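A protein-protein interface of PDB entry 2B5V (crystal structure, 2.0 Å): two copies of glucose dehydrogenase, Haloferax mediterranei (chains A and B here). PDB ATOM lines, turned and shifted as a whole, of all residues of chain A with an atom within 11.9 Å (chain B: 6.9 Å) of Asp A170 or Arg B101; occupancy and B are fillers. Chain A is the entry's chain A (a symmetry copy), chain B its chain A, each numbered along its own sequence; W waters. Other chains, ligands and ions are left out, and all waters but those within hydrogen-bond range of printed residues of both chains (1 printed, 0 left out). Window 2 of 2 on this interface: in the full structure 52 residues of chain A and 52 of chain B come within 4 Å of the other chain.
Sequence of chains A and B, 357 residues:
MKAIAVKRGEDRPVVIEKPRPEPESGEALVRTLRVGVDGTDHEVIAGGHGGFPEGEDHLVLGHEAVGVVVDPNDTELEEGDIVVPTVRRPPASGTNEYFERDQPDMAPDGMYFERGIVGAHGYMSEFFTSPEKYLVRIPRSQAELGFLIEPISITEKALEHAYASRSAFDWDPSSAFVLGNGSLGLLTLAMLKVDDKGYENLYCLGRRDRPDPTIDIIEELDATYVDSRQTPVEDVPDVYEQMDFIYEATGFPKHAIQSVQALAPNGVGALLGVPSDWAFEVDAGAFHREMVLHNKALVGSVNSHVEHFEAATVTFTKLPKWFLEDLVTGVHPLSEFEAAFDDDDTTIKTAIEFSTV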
ATOM      1  N   ALA A 162      21.336  -4.188 -13.301  1.00  0.00           N
ATOM      2  CA  ALA A 162      20.898  -4.577 -11.978  1.00  0.00           C
ATOM      3  C   ALA A 162      20.898  -3.359 -11.053  1.00  0.00           C
ATOM      4  O   ALA A 162      19.952  -3.173 -10.298  1.00  0.00           O
ATOM      5  CB  ALA A 162      21.786  -5.646 -11.436  1.00  0.00           C
ATOM      6  N   TYR A 163      21.958  -2.546 -11.098  1.00  0.00           N
ATOM      7  CA  TYR A 163      22.010  -1.358 -10.260  1.00  0.00           C
ATOM      8  C   TYR A 163      20.943  -0.330 -10.664  1.00  0.00           C
ATOM      9  O   TYR A 163      20.374   0.345  -9.797  1.00  0.00           O
ATOM     10  CB  TYR A 163      23.410  -0.725 -10.304  1.00  0.00           C
ATOM     11  CG  TYR A 163      24.492  -1.597  -9.679  1.00  0.00           C
ATOM     12  CD1 TYR A 163      24.170  -2.765  -8.951  1.00  0.00           C
ATOM     13  CD2 TYR A 163      25.844  -1.254  -9.810  1.00  0.00           C
ATOM     14  CE1 TYR A 163      25.179  -3.564  -8.374  1.00  0.00           C
ATOM     15  CE2 TYR A 163      26.844  -2.036  -9.248  1.00  0.00           C
ATOM     16  CZ  TYR A 163      26.520  -3.182  -8.533  1.00  0.00           C
ATOM     17  OH  TYR A 163      27.551  -3.930  -7.984  1.00  0.00           O
ATOM     18  N   ALA A 164      20.647  -0.230 -11.963  1.00  0.00           N
ATOM     19  CA  ALA A 164      19.622   0.723 -12.413  1.00  0.00           C
ATOM     20  C   ALA A 164      18.253   0.340 -11.809  1.00  0.00           C
ATOM     21  O   ALA A 164      17.426   1.210 -11.545  1.00  0.00           O
ATOM     22  CB  ALA A 164      19.539   0.758 -13.998  1.00  0.00           C
ATOM     23  N   SER A 165      18.020  -0.953 -11.570  1.00  0.00           N
ATOM     24  CA  SER A 165      16.739  -1.393 -11.001  1.00  0.00           C
ATOM     25  C   SER A 165      16.564  -0.975  -9.531  1.00  0.00           C
ATOM     26  O   SER A 165      15.442  -0.961  -9.015  1.00  0.00           O
ATOM     27  CB  SER A 165      16.595  -2.915 -11.100  1.00  0.00           C
ATOM     28  OG  SER A 165      17.287  -3.535 -10.049  1.00  0.00           O
ATOM     29  N   ARG A 166      17.669  -0.649  -8.862  1.00  0.00           N
ATOM     30  CA  ARG A 166      17.620  -0.224  -7.457  1.00  0.00           C
ATOM     31  C   ARG A 166      17.796   1.295  -7.359  1.00  0.00           C
ATOM     32  O   ARG A 166      17.949   1.820  -6.264  1.00  0.00           O
ATOM     33  CB  ARG A 166      18.771  -0.860  -6.627  1.00  0.00           C
ATOM     34  CG  ARG A 166      18.865  -2.390  -6.686  1.00  0.00           C
ATOM     35  CD  ARG A 166      17.633  -3.098  -6.096  1.00  0.00           C
ATOM     36  NE  ARG A 166      16.441  -3.085  -6.960  1.00  0.00           N
ATOM     37  CZ  ARG A 166      15.207  -3.329  -6.501  1.00  0.00           C
ATOM     38  NH1 ARG A 166      14.137  -3.292  -7.301  1.00  0.00           N
ATOM     39  NH2 ARG A 166      15.046  -3.638  -5.226  1.00  0.00           N
ATOM     40  N   SER A 167      17.756   2.003  -8.478  1.00  0.00           N
ATOM     41  CA  SER A 167      17.988   3.444  -8.430  1.00  0.00           C
ATOM     42  C   SER A 167      16.861   4.338  -7.961  1.00  0.00           C
ATOM     43  O   SER A 167      17.087   5.536  -7.789  1.00  0.00           O
ATOM     44  CB  SER A 167      18.493   3.974  -9.783  1.00  0.00           C
ATOM     45  OG  SER A 167      17.537   3.737 -10.798  1.00  0.00           O
ATOM     46  N   ALA A 168      15.665   3.796  -7.727  1.00  0.00           N
ATOM     47  CA  ALA A 168      14.581   4.672  -7.281  1.00  0.00           C
ATOM     48  C   ALA A 168      14.596   4.870  -5.780  1.00  0.00           C
ATOM     49  O   ALA A 168      13.747   5.581  -5.245  1.00  0.00           O
ATOM     50  CB  ALA A 168      13.197   4.147  -7.740  1.00  0.00           C
ATOM     51  N   PHE A 169      15.516   4.209  -5.083  1.00  0.00           N
ATOM     52  CA  PHE A 169      15.627   4.412  -3.639  1.00  0.00           C
ATOM     53  C   PHE A 169      17.092   4.368  -3.208  1.00  0.00           C
ATOM     54  O   PHE A 169      17.979   4.055  -4.026  1.00  0.00           O
ATOM     55  CB  PHE A 169      14.809   3.381  -2.844  1.00  0.00           C
ATOM     56  CG  PHE A 169      15.369   1.980  -2.897  1.00  0.00           C
ATOM     57  CD1 PHE A 169      15.995   1.431  -1.786  1.00  0.00           C
ATOM     58  CD2 PHE A 169      15.264   1.220  -4.059  1.00  0.00           C
ATOM     59  CE1 PHE A 169      16.514   0.132  -1.819  1.00  0.00           C
ATOM     60  CE2 PHE A 169      15.775  -0.087  -4.119  1.00  0.00           C
ATOM     61  CZ  PHE A 169      16.403  -0.632  -2.996  1.00  0.00           C
ATOM     62  N   ASP A 170      17.345   4.675  -1.931  1.00  0.00           N
ATOM     63  CA  ASP A 170      18.719   4.672  -1.392  1.00  0.00           C
ATOM     64  C   ASP A 170      19.125   3.245  -1.064  1.00  0.00           C
ATOM     65  O   ASP A 170      18.791   2.712  -0.011  1.00  0.00           O
ATOM     66  CB  ASP A 170      18.808   5.527  -0.131  1.00  0.00           C
ATOM     67  CG  ASP A 170      19.368   6.903  -0.404  1.00  0.00           C
ATOM     68  OD1 ASP A 170      20.607   7.070  -0.326  1.00  0.00           O
ATOM     69  OD2 ASP A 170      18.568   7.811  -0.712  1.00  0.00           O
ATOM     70  N   TRP A 171      19.832   2.610  -1.984  1.00  0.00           N
ATOM     71  CA  TRP A 171      20.244   1.228  -1.751  1.00  0.00           C
ATOM     72  C   TRP A 171      21.731   1.218  -1.380  1.00  0.00           C
ATOM     73  O   TRP A 171      22.542   1.788  -2.076  1.00  0.00           O
ATOM     74  CB  TRP A 171      20.021   0.415  -3.023  1.00  0.00           C
ATOM     75  CG  TRP A 171      20.341  -1.038  -2.926  1.00  0.00           C
ATOM     76  CD1 TRP A 171      19.764  -1.948  -2.086  1.00  0.00           C
ATOM     77  CD2 TRP A 171      21.204  -1.781  -3.801  1.00  0.00           C
ATOM     78  NE1 TRP A 171      20.206  -3.219  -2.396  1.00  0.00           N
ATOM     79  CE2 TRP A 171      21.086  -3.141  -3.445  1.00  0.00           C
ATOM     80  CE3 TRP A 171      22.062  -1.424  -4.862  1.00  0.00           C
ATOM     81  CZ2 TRP A 171      21.785  -4.156  -4.111  1.00  0.00           C
ATOM     82  CZ3 TRP A 171      22.758  -2.437  -5.528  1.00  0.00           C
ATOM     83  CH2 TRP A 171      22.611  -3.790  -5.146  1.00  0.00           C
ATOM     84  N   ASP A 172      22.070   0.561  -0.287  1.00  0.00           N
ATOM     85  CA  ASP A 172      23.464   0.479   0.147  1.00  0.00           C
ATOM     86  C   ASP A 172      23.762  -0.977   0.512  1.00  0.00           C
ATOM     87  O   ASP A 172      23.628  -1.382   1.664  1.00  0.00           O
ATOM     88  CB  ASP A 172      23.683   1.388   1.357  1.00  0.00           C
ATOM     89  CG  ASP A 172      25.131   1.425   1.797  1.00  0.00           C
ATOM     90  OD1 ASP A 172      26.029   1.455   0.916  1.00  0.00           O
ATOM     91  OD2 ASP A 172      25.366   1.435   3.024  1.00  0.00           O
ATOM     92  N   PRO A 173      24.160  -1.785  -0.479  1.00  0.00           N
ATOM     93  CA  PRO A 173      24.453  -3.192  -0.229  1.00  0.00           C
ATOM     94  C   PRO A 173      25.749  -3.398   0.540  1.00  0.00           C
ATOM     95  O   PRO A 173      26.645  -2.567   0.477  1.00  0.00           O
ATOM     96  CB  PRO A 173      24.524  -3.766  -1.632  1.00  0.00           C
ATOM     97  CG  PRO A 173      25.243  -2.635  -2.380  1.00  0.00           C
ATOM     98  CD  PRO A 173      24.445  -1.424  -1.879  1.00  0.00           C
ATOM     99  N   SER A 174      25.844  -4.514   1.253  1.00  0.00           N
ATOM    100  CA  SER A 174      27.060  -4.828   1.984  1.00  0.00           C
ATOM    101  C   SER A 174      27.519  -6.242   1.586  1.00  0.00           C
ATOM    102  O   SER A 174      28.712  -6.549   1.629  1.00  0.00           O
ATOM    103  CB  SER A 174      26.794  -4.764   3.493  1.00  0.00           C
ATOM    104  OG  SER A 174      25.891  -5.785   3.858  1.00  0.00           O
ATOM    105  N   LYS A 197      30.451   0.071  -5.025  1.00  0.00           N
ATOM    106  CA  LYS A 197      29.347  -0.111  -4.068  1.00  0.00           C
ATOM    107  C   LYS A 197      29.871  -0.548  -2.699  1.00  0.00           C
ATOM    108  O   LYS A 197      29.111  -0.643  -1.732  1.00  0.00           O
ATOM    109  CB  LYS A 197      28.342  -1.156  -4.561  1.00  0.00           C
ATOM    110  CG  LYS A 197      27.505  -0.731  -5.752  1.00  0.00           C
ATOM    111  CD  LYS A 197      26.241  -0.060  -5.326  1.00  0.00           C
ATOM    112  CE  LYS A 197      25.516   0.519  -6.540  1.00  0.00           C
ATOM    113  NZ  LYS A 197      26.403   1.446  -7.292  1.00  0.00           N
ATOM    114  N   ASP A 244      22.591  -9.005  -0.408  1.00  0.00           N
ATOM    115  CA  ASP A 244      22.036  -7.843  -1.083  1.00  0.00           C
ATOM    116  C   ASP A 244      22.052  -7.970  -2.594  1.00  0.00           C
ATOM    117  O   ASP A 244      21.148  -7.481  -3.281  1.00  0.00           O
ATOM    118  CB  ASP A 244      22.799  -6.594  -0.678  1.00  0.00           C
ATOM    119  CG  ASP A 244      22.607  -6.273   0.791  1.00  0.00           C
ATOM    120  OD1 ASP A 244      21.430  -6.170   1.211  1.00  0.00           O
ATOM    121  OD2 ASP A 244      23.626  -6.136   1.511  1.00  0.00           O
ATOM    122  N   ALA A 264      18.492 -10.459   0.296  1.00  0.00           N
ATOM    123  CA  ALA A 264      18.077  -9.654   1.428  1.00  0.00           C
ATOM    124  C   ALA A 264      16.921  -8.756   0.922  1.00  0.00           C
ATOM    125  O   ALA A 264      16.704  -8.617  -0.282  1.00  0.00           O
ATOM    126  CB  ALA A 264      19.241  -8.773   1.900  1.00  0.00           C
ATOM    127  N   PRO A 265      16.146  -8.167   1.840  1.00  0.00           N
ATOM    128  CA  PRO A 265      15.044  -7.290   1.429  1.00  0.00           C
ATOM    129  C   PRO A 265      15.636  -6.191   0.554  1.00  0.00           C
ATOM    130  O   PRO A 265      16.758  -5.705   0.818  1.00  0.00           O
ATOM    131  CB  PRO A 265      14.528  -6.748   2.763  1.00  0.00           C
ATOM    132  CG  PRO A 265      14.705  -7.956   3.664  1.00  0.00           C
ATOM    133  CD  PRO A 265      16.115  -8.409   3.292  1.00  0.00           C
ATOM    134  N   ASN A 266      14.903  -5.826  -0.498  1.00  0.00           N
ATOM    135  CA  ASN A 266      15.305  -4.773  -1.433  1.00  0.00           C
ATOM    136  C   ASN A 266      16.510  -5.144  -2.306  1.00  0.00           C
ATOM    137  O   ASN A 266      17.052  -4.298  -3.013  1.00  0.00           O
ATOM    138  CB  ASN A 266      15.601  -3.481  -0.668  1.00  0.00           C
ATOM    139  CG  ASN A 266      14.495  -3.140   0.324  1.00  0.00           C
ATOM    140  OD1 ASN A 266      13.308  -3.368   0.048  1.00  0.00           O
ATOM    141  ND2 ASN A 266      14.871  -2.609   1.480  1.00  0.00           N
ATOM    142  N   GLY A 267      16.893  -6.414  -2.284  1.00  0.00           N
ATOM    143  CA  GLY A 267      18.033  -6.847  -3.082  1.00  0.00           C
ATOM    144  C   GLY A 267      17.680  -7.116  -4.540  1.00  0.00           C
ATOM    145  O   GLY A 267      16.500  -7.066  -4.921  1.00  0.00           O
ATOM    146  N   VAL A 268      18.696  -7.378  -5.369  1.00  0.00           N
ATOM    147  CA  VAL A 268      18.450  -7.680  -6.773  1.00  0.00           C
ATOM    148  C   VAL A 268      19.340  -8.838  -7.184  1.00  0.00           C
ATOM    149  O   VAL A 268      20.487  -8.968  -6.692  1.00  0.00           O
ATOM    150  CB  VAL A 268      18.738  -6.453  -7.722  1.00  0.00           C
ATOM    151  CG1 VAL A 268      20.093  -5.832  -7.415  1.00  0.00           C
ATOM    152  CG2 VAL A 268      18.705  -6.889  -9.206  1.00  0.00           C
ATOM    153  N   HIS A 294       9.066  -7.886  -0.133  1.00  0.00           N
ATOM    154  CA  HIS A 294      10.400  -7.385   0.155  1.00  0.00           C
ATOM    155  C   HIS A 294      11.044  -6.562  -0.966  1.00  0.00           C
ATOM    156  O   HIS A 294      12.272  -6.418  -1.012  1.00  0.00           O
ATOM    157  CB  HIS A 294      11.313  -8.542   0.616  1.00  0.00           C
ATOM    158  CG  HIS A 294      11.055  -8.943   2.035  1.00  0.00           C
ATOM    159  ND1 HIS A 294      10.800  -8.016   3.026  1.00  0.00           N
ATOM    160  CD2 HIS A 294      10.957 -10.158   2.625  1.00  0.00           C
ATOM    161  CE1 HIS A 294      10.553  -8.640   4.164  1.00  0.00           C
ATOM    162  NE2 HIS A 294      10.640  -9.942   3.945  1.00  0.00           N
ATOM    163  N   ASN A 295      10.203  -6.008  -1.845  1.00  0.00           N
ATOM    164  CA  ASN A 295      10.657  -5.126  -2.922  1.00  0.00           C
ATOM    165  C   ASN A 295      11.901  -5.676  -3.615  1.00  0.00           C
ATOM    166  O   ASN A 295      12.904  -4.981  -3.688  1.00  0.00           O
ATOM    167  CB  ASN A 295      11.015  -3.733  -2.350  1.00  0.00           C
ATOM    168  CG  ASN A 295       9.822  -3.041  -1.675  1.00  0.00           C
ATOM    169  OD1 ASN A 295       8.925  -2.543  -2.349  1.00  0.00           O
ATOM    170  ND2 ASN A 295       9.807  -3.021  -0.330  1.00  0.00           N
ATOM    171  N   THR B  95      11.747   3.888  15.926  1.00  0.00           N
ATOM    172  CA  THR B  95      12.216   4.161  14.586  1.00  0.00           C
ATOM    173  C   THR B  95      13.382   3.257  14.187  1.00  0.00           C
ATOM    174  O   THR B  95      13.869   2.469  14.979  1.00  0.00           O
ATOM    175  CB  THR B  95      12.655   5.626  14.496  1.00  0.00           C
ATOM    176  OG1 THR B  95      12.999   5.953  13.146  1.00  0.00           O
ATOM    177  CG2 THR B  95      13.855   5.861  15.403  1.00  0.00           C
ATOM    178  N   ASN B  96      13.792   3.365  12.931  1.00  0.00           N
ATOM    179  CA  ASN B  96      14.907   2.607  12.384  1.00  0.00           C
ATOM    180  C   ASN B  96      15.359   3.332  11.134  1.00  0.00           C
ATOM    181  O   ASN B  96      14.796   4.370  10.782  1.00  0.00           O
ATOM    182  CB  ASN B  96      14.526   1.151  12.063  1.00  0.00           C
ATOM    183  CG  ASN B  96      13.338   1.032  11.096  1.00  0.00           C
ATOM    184  OD1 ASN B  96      13.252   1.738  10.087  1.00  0.00           O
ATOM    185  ND2 ASN B  96      12.435   0.116  11.401  1.00  0.00           N
ATOM    186  N   GLU B  97      16.364   2.787  10.460  1.00  0.00           N
ATOM    187  CA  GLU B  97      16.915   3.417   9.271  1.00  0.00           C
ATOM    188  C   GLU B  97      15.901   3.692   8.148  1.00  0.00           C
ATOM    189  O   GLU B  97      15.992   4.705   7.438  1.00  0.00           O
ATOM    190  CB  GLU B  97      18.065   2.560   8.716  1.00  0.00           C
ATOM    191  CG  GLU B  97      17.592   1.321   7.961  1.00  0.00           C
ATOM    192  CD  GLU B  97      18.728   0.545   7.315  1.00  0.00           C
ATOM    193  OE1 GLU B  97      19.577   0.011   8.057  1.00  0.00           O
ATOM    194  OE2 GLU B  97      18.771   0.470   6.064  1.00  0.00           O
ATOM    195  N   TYR B  98      14.948   2.791   7.958  1.00  0.00           N
ATOM    196  CA  TYR B  98      13.968   3.022   6.902  1.00  0.00           C
ATOM    197  C   TYR B  98      13.133   4.261   7.166  1.00  0.00           C
ATOM    198  O   TYR B  98      12.837   5.035   6.248  1.00  0.00           O
ATOM    199  CB  TYR B  98      13.103   1.786   6.744  1.00  0.00           C
ATOM    200  CG  TYR B  98      13.949   0.638   6.263  1.00  0.00           C
ATOM    201  CD1 TYR B  98      14.412  -0.337   7.147  1.00  0.00           C
ATOM    202  CD2 TYR B  98      14.353   0.572   4.925  1.00  0.00           C
ATOM    203  CE1 TYR B  98      15.257  -1.352   6.710  1.00  0.00           C
ATOM    204  CE2 TYR B  98      15.199  -0.435   4.482  1.00  0.00           C
ATOM    205  CZ  TYR B  98      15.645  -1.389   5.381  1.00  0.00           C
ATOM    206  OH  TYR B  98      16.490  -2.374   4.949  1.00  0.00           O
ATOM    207  N   PHE B  99      12.766   4.475   8.422  1.00  0.00           N
ATOM    208  CA  PHE B  99      11.988   5.650   8.738  1.00  0.00           C
ATOM    209  C   PHE B  99      12.922   6.870   8.838  1.00  0.00           C
ATOM    210  O   PHE B  99      12.569   7.972   8.407  1.00  0.00           O
ATOM    211  CB  PHE B  99      11.190   5.418  10.022  1.00  0.00           C
ATOM    212  CG  PHE B  99       9.999   4.510   9.839  1.00  0.00           C
ATOM    213  CD1 PHE B  99      10.131   3.126   9.935  1.00  0.00           C
ATOM    214  CD2 PHE B  99       8.748   5.044   9.559  1.00  0.00           C
ATOM    215  CE1 PHE B  99       9.025   2.290   9.753  1.00  0.00           C
ATOM    216  CE2 PHE B  99       7.630   4.223   9.380  1.00  0.00           C
ATOM    217  CZ  PHE B  99       7.763   2.845   9.475  1.00  0.00           C
ATOM    218  N   GLU B 100      14.136   6.657   9.345  1.00  0.00           N
ATOM    219  CA  GLU B 100      15.106   7.749   9.480  1.00  0.00           C
ATOM    220  C   GLU B 100      15.393   8.427   8.157  1.00  0.00           C
ATOM    221  O   GLU B 100      15.357   9.657   8.045  1.00  0.00           O
ATOM    222  CB  GLU B 100      16.402   7.220  10.068  1.00  0.00           C
ATOM    223  CG  GLU B 100      16.274   6.859  11.532  1.00  0.00           C
ATOM    224  CD  GLU B 100      16.097   8.087  12.393  1.00  0.00           C
ATOM    225  OE1 GLU B 100      17.086   8.837  12.549  1.00  0.00           O
ATOM    226  OE2 GLU B 100      14.974   8.310  12.899  1.00  0.00           O
ATOM    227  N   ARG B 101      15.656   7.604   7.147  1.00  0.00           N
ATOM    228  CA  ARG B 101      15.955   8.072   5.801  1.00  0.00           C
ATOM    229  C   ARG B 101      14.729   8.372   4.964  1.00  0.00           C
ATOM    230  O   ARG B 101      14.854   8.715   3.790  1.00  0.00           O
ATOM    231  CB  ARG B 101      16.776   7.025   5.061  1.00  0.00           C
ATOM    232  CG  ARG B 101      18.188   6.842   5.573  1.00  0.00           C
ATOM    233  CD  ARG B 101      18.904   5.779   4.739  1.00  0.00           C
ATOM    234  NE  ARG B 101      20.358   5.852   4.868  1.00  0.00           N
ATOM    235  CZ  ARG B 101      21.115   6.791   4.309  1.00  0.00           C
ATOM    236  NH1 ARG B 101      20.556   7.745   3.571  1.00  0.00           N
ATOM    237  NH2 ARG B 101      22.431   6.783   4.492  1.00  0.00           N
ATOM    238  N   ASP B 102      13.545   8.218   5.547  1.00  0.00           N
ATOM    239  CA  ASP B 102      12.308   8.477   4.814  1.00  0.00           C
ATOM    240  C   ASP B 102      11.954   7.501   3.698  1.00  0.00           C
ATOM    241  O   ASP B 102      11.453   7.925   2.649  1.00  0.00           O
ATOM    242  CB  ASP B 102      12.308   9.889   4.213  1.00  0.00           C
ATOM    243  CG  ASP B 102      12.133  10.959   5.250  1.00  0.00           C
ATOM    244  OD1 ASP B 102      11.123  10.911   5.982  1.00  0.00           O
ATOM    245  OD2 ASP B 102      13.004  11.847   5.329  1.00  0.00           O
ATOM    246  N   GLN B 103      12.203   6.211   3.906  1.00  0.00           N
ATOM    247  CA  GLN B 103      11.827   5.207   2.912  1.00  0.00           C
ATOM    248  C   GLN B 103      11.126   4.078   3.663  1.00  0.00           C
ATOM    249  O   GLN B 103      11.510   2.923   3.516  1.00  0.00           O
ATOM    250  CB  GLN B 103      13.049   4.571   2.198  1.00  0.00           C
ATOM    251  CG  GLN B 103      14.329   5.355   2.109  1.00  0.00           C
ATOM    252  CD  GLN B 103      15.378   4.648   1.222  1.00  0.00           C
ATOM    253  OE1 GLN B 103      16.028   3.658   1.620  1.00  0.00           O
ATOM    254  NE2 GLN B 103      15.533   5.158   0.011  1.00  0.00           N
ATOM    255  N   PRO B 104      10.095   4.383   4.476  1.00  0.00           N
ATOM    256  CA  PRO B 104       9.451   3.265   5.185  1.00  0.00           C
ATOM    257  C   PRO B 104       8.798   2.227   4.266  1.00  0.00           C
ATOM    258  O   PRO B 104       8.565   1.080   4.660  1.00  0.00           O
ATOM    259  CB  PRO B 104       8.439   3.953   6.111  1.00  0.00           C
ATOM    260  CG  PRO B 104       8.125   5.265   5.419  1.00  0.00           C
ATOM    261  CD  PRO B 104       9.490   5.686   4.839  1.00  0.00           C
ATOM    262  N   MET B 106      10.140   0.806   1.992  1.00  0.00           N
ATOM    263  CA  MET B 106      11.162  -0.200   1.677  1.00  0.00           C
ATOM    264  C   MET B 106      11.534  -1.021   2.909  1.00  0.00           C
ATOM    265  O   MET B 106      12.420  -1.867   2.834  1.00  0.00           O
ATOM    266  CB  MET B 106      12.463   0.456   1.151  1.00  0.00           C
ATOM    267  CG  MET B 106      12.292   1.355  -0.089  1.00  0.00           C
ATOM    268  SD  MET B 106      11.585   0.485  -1.494  1.00  0.00           S
ATOM    269  CE  MET B 106      13.020  -0.485  -1.911  1.00  0.00           C
HETATM  270  O   HOH W   1      11.537  -4.585   1.885  1.00  0.00           O
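The side-chain amide nitrogen of Gln B103 lies close to the backbone NH of Asp A170 (2.7 Å). O of Met B106 is in hydrogen-bond range of ND2 of Asn A266, 2.9 Å away. The guanidinium group of Arg B101 is in salt-bridge range of the side-chain carboxylate of Asp A170 (3.96 Å).
The backbone carbonyl oxygen (O) of Asn A266 lies within hydrogen-bond range of the guanidinium group (NH2) of Arg A166. The guanidinium group of Arg A166 sits at hydrogen-bond distance from the backbone carbonyl oxygen of Asn A295 (3.0 Å). N of Asn A266 lies within hydrogen-bond range of O of His A294, at 2.7 Å. The backbone carbonyl oxygen (O) of Asn A266 lies within hydrogen-bond range of the indole nitrogen (NE1) of Trp A171 (3.4 Å). The side-chain amide oxygen of Asn B96 sits at hydrogen-bond distance from the backbone NH of Tyr B98 (2.9 Å). N of Gln B103 sits at hydrogen-bond distance from O of Tyr B98 (2.7 Å).
Among the printed residues, merely in contact across the chains: Phe A169 with Gln B103 (3.4 Å), Phe A169 with Met B106 (3.5 Å), Asn A295 with Met B106 (3.7 Å) and Asn A266 with Tyr B98 (3.7 Å).
Printed residues of chain A within 4 Å of Arg B101: Asp A170 (3.96 Å). No residue of chain A comes within 4 Å of Glu B97. No residue of chain A comes within 4 Å of Glu B100. No residue of chain A comes within 4 Å of Asp B102. Of the printed residues of chain A, Gln B103 touches Phe A169 (3.4 Å) and Asp A170 (2.7 Å). Of the printed residues of chain B, Asn A295 touches Met B106. Printed residues of chain A within 4 Å of Met B106: Phe A169 (3.5 Å), Asn A266 (2.9 Å) and Asn A295 (3.7 Å). Printed residues of chain A within 4 Å of Tyr B98: Asn A266 (3.7 Å). Of the printed residues of chain B, Asn A266 touches Tyr B98 and Met B106. Printed residues of chain B within 4 Å of Phe A169: Gln B103 (3.4 Å) and Met B106 (3.5 Å). Ala A264 touches none of the printed residues of chain B. Ser A167 touches none of the printed residues of chain B. The nearest residue of chain A that does not touch Arg B101 is Asp A172 (6.3 Å).
Hydrophobic or aromatic side chains of chain B within 4 Å of the printed part of chain A: Tyr B98 and Met B106. Hydrophobic or aromatic side chains of chain A that line the printed part of chain B: Phe A169. Among the printed residues, Asp or Glu carboxylates within 4 Å of a Lys or Arg side-chain nitrogen of the other chain: Asp A170 with Arg B101 (3.96 Å).
No position is printed for both chains.
Water W1 lies within hydrogen-bond range of the side-chain amide oxygen of Asn A266 (2.8 Å), the backbone carbonyl oxygen of Met B106 (3.0 Å) and the side-chain amide nitrogen of Asn A295 (3.2 Å).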
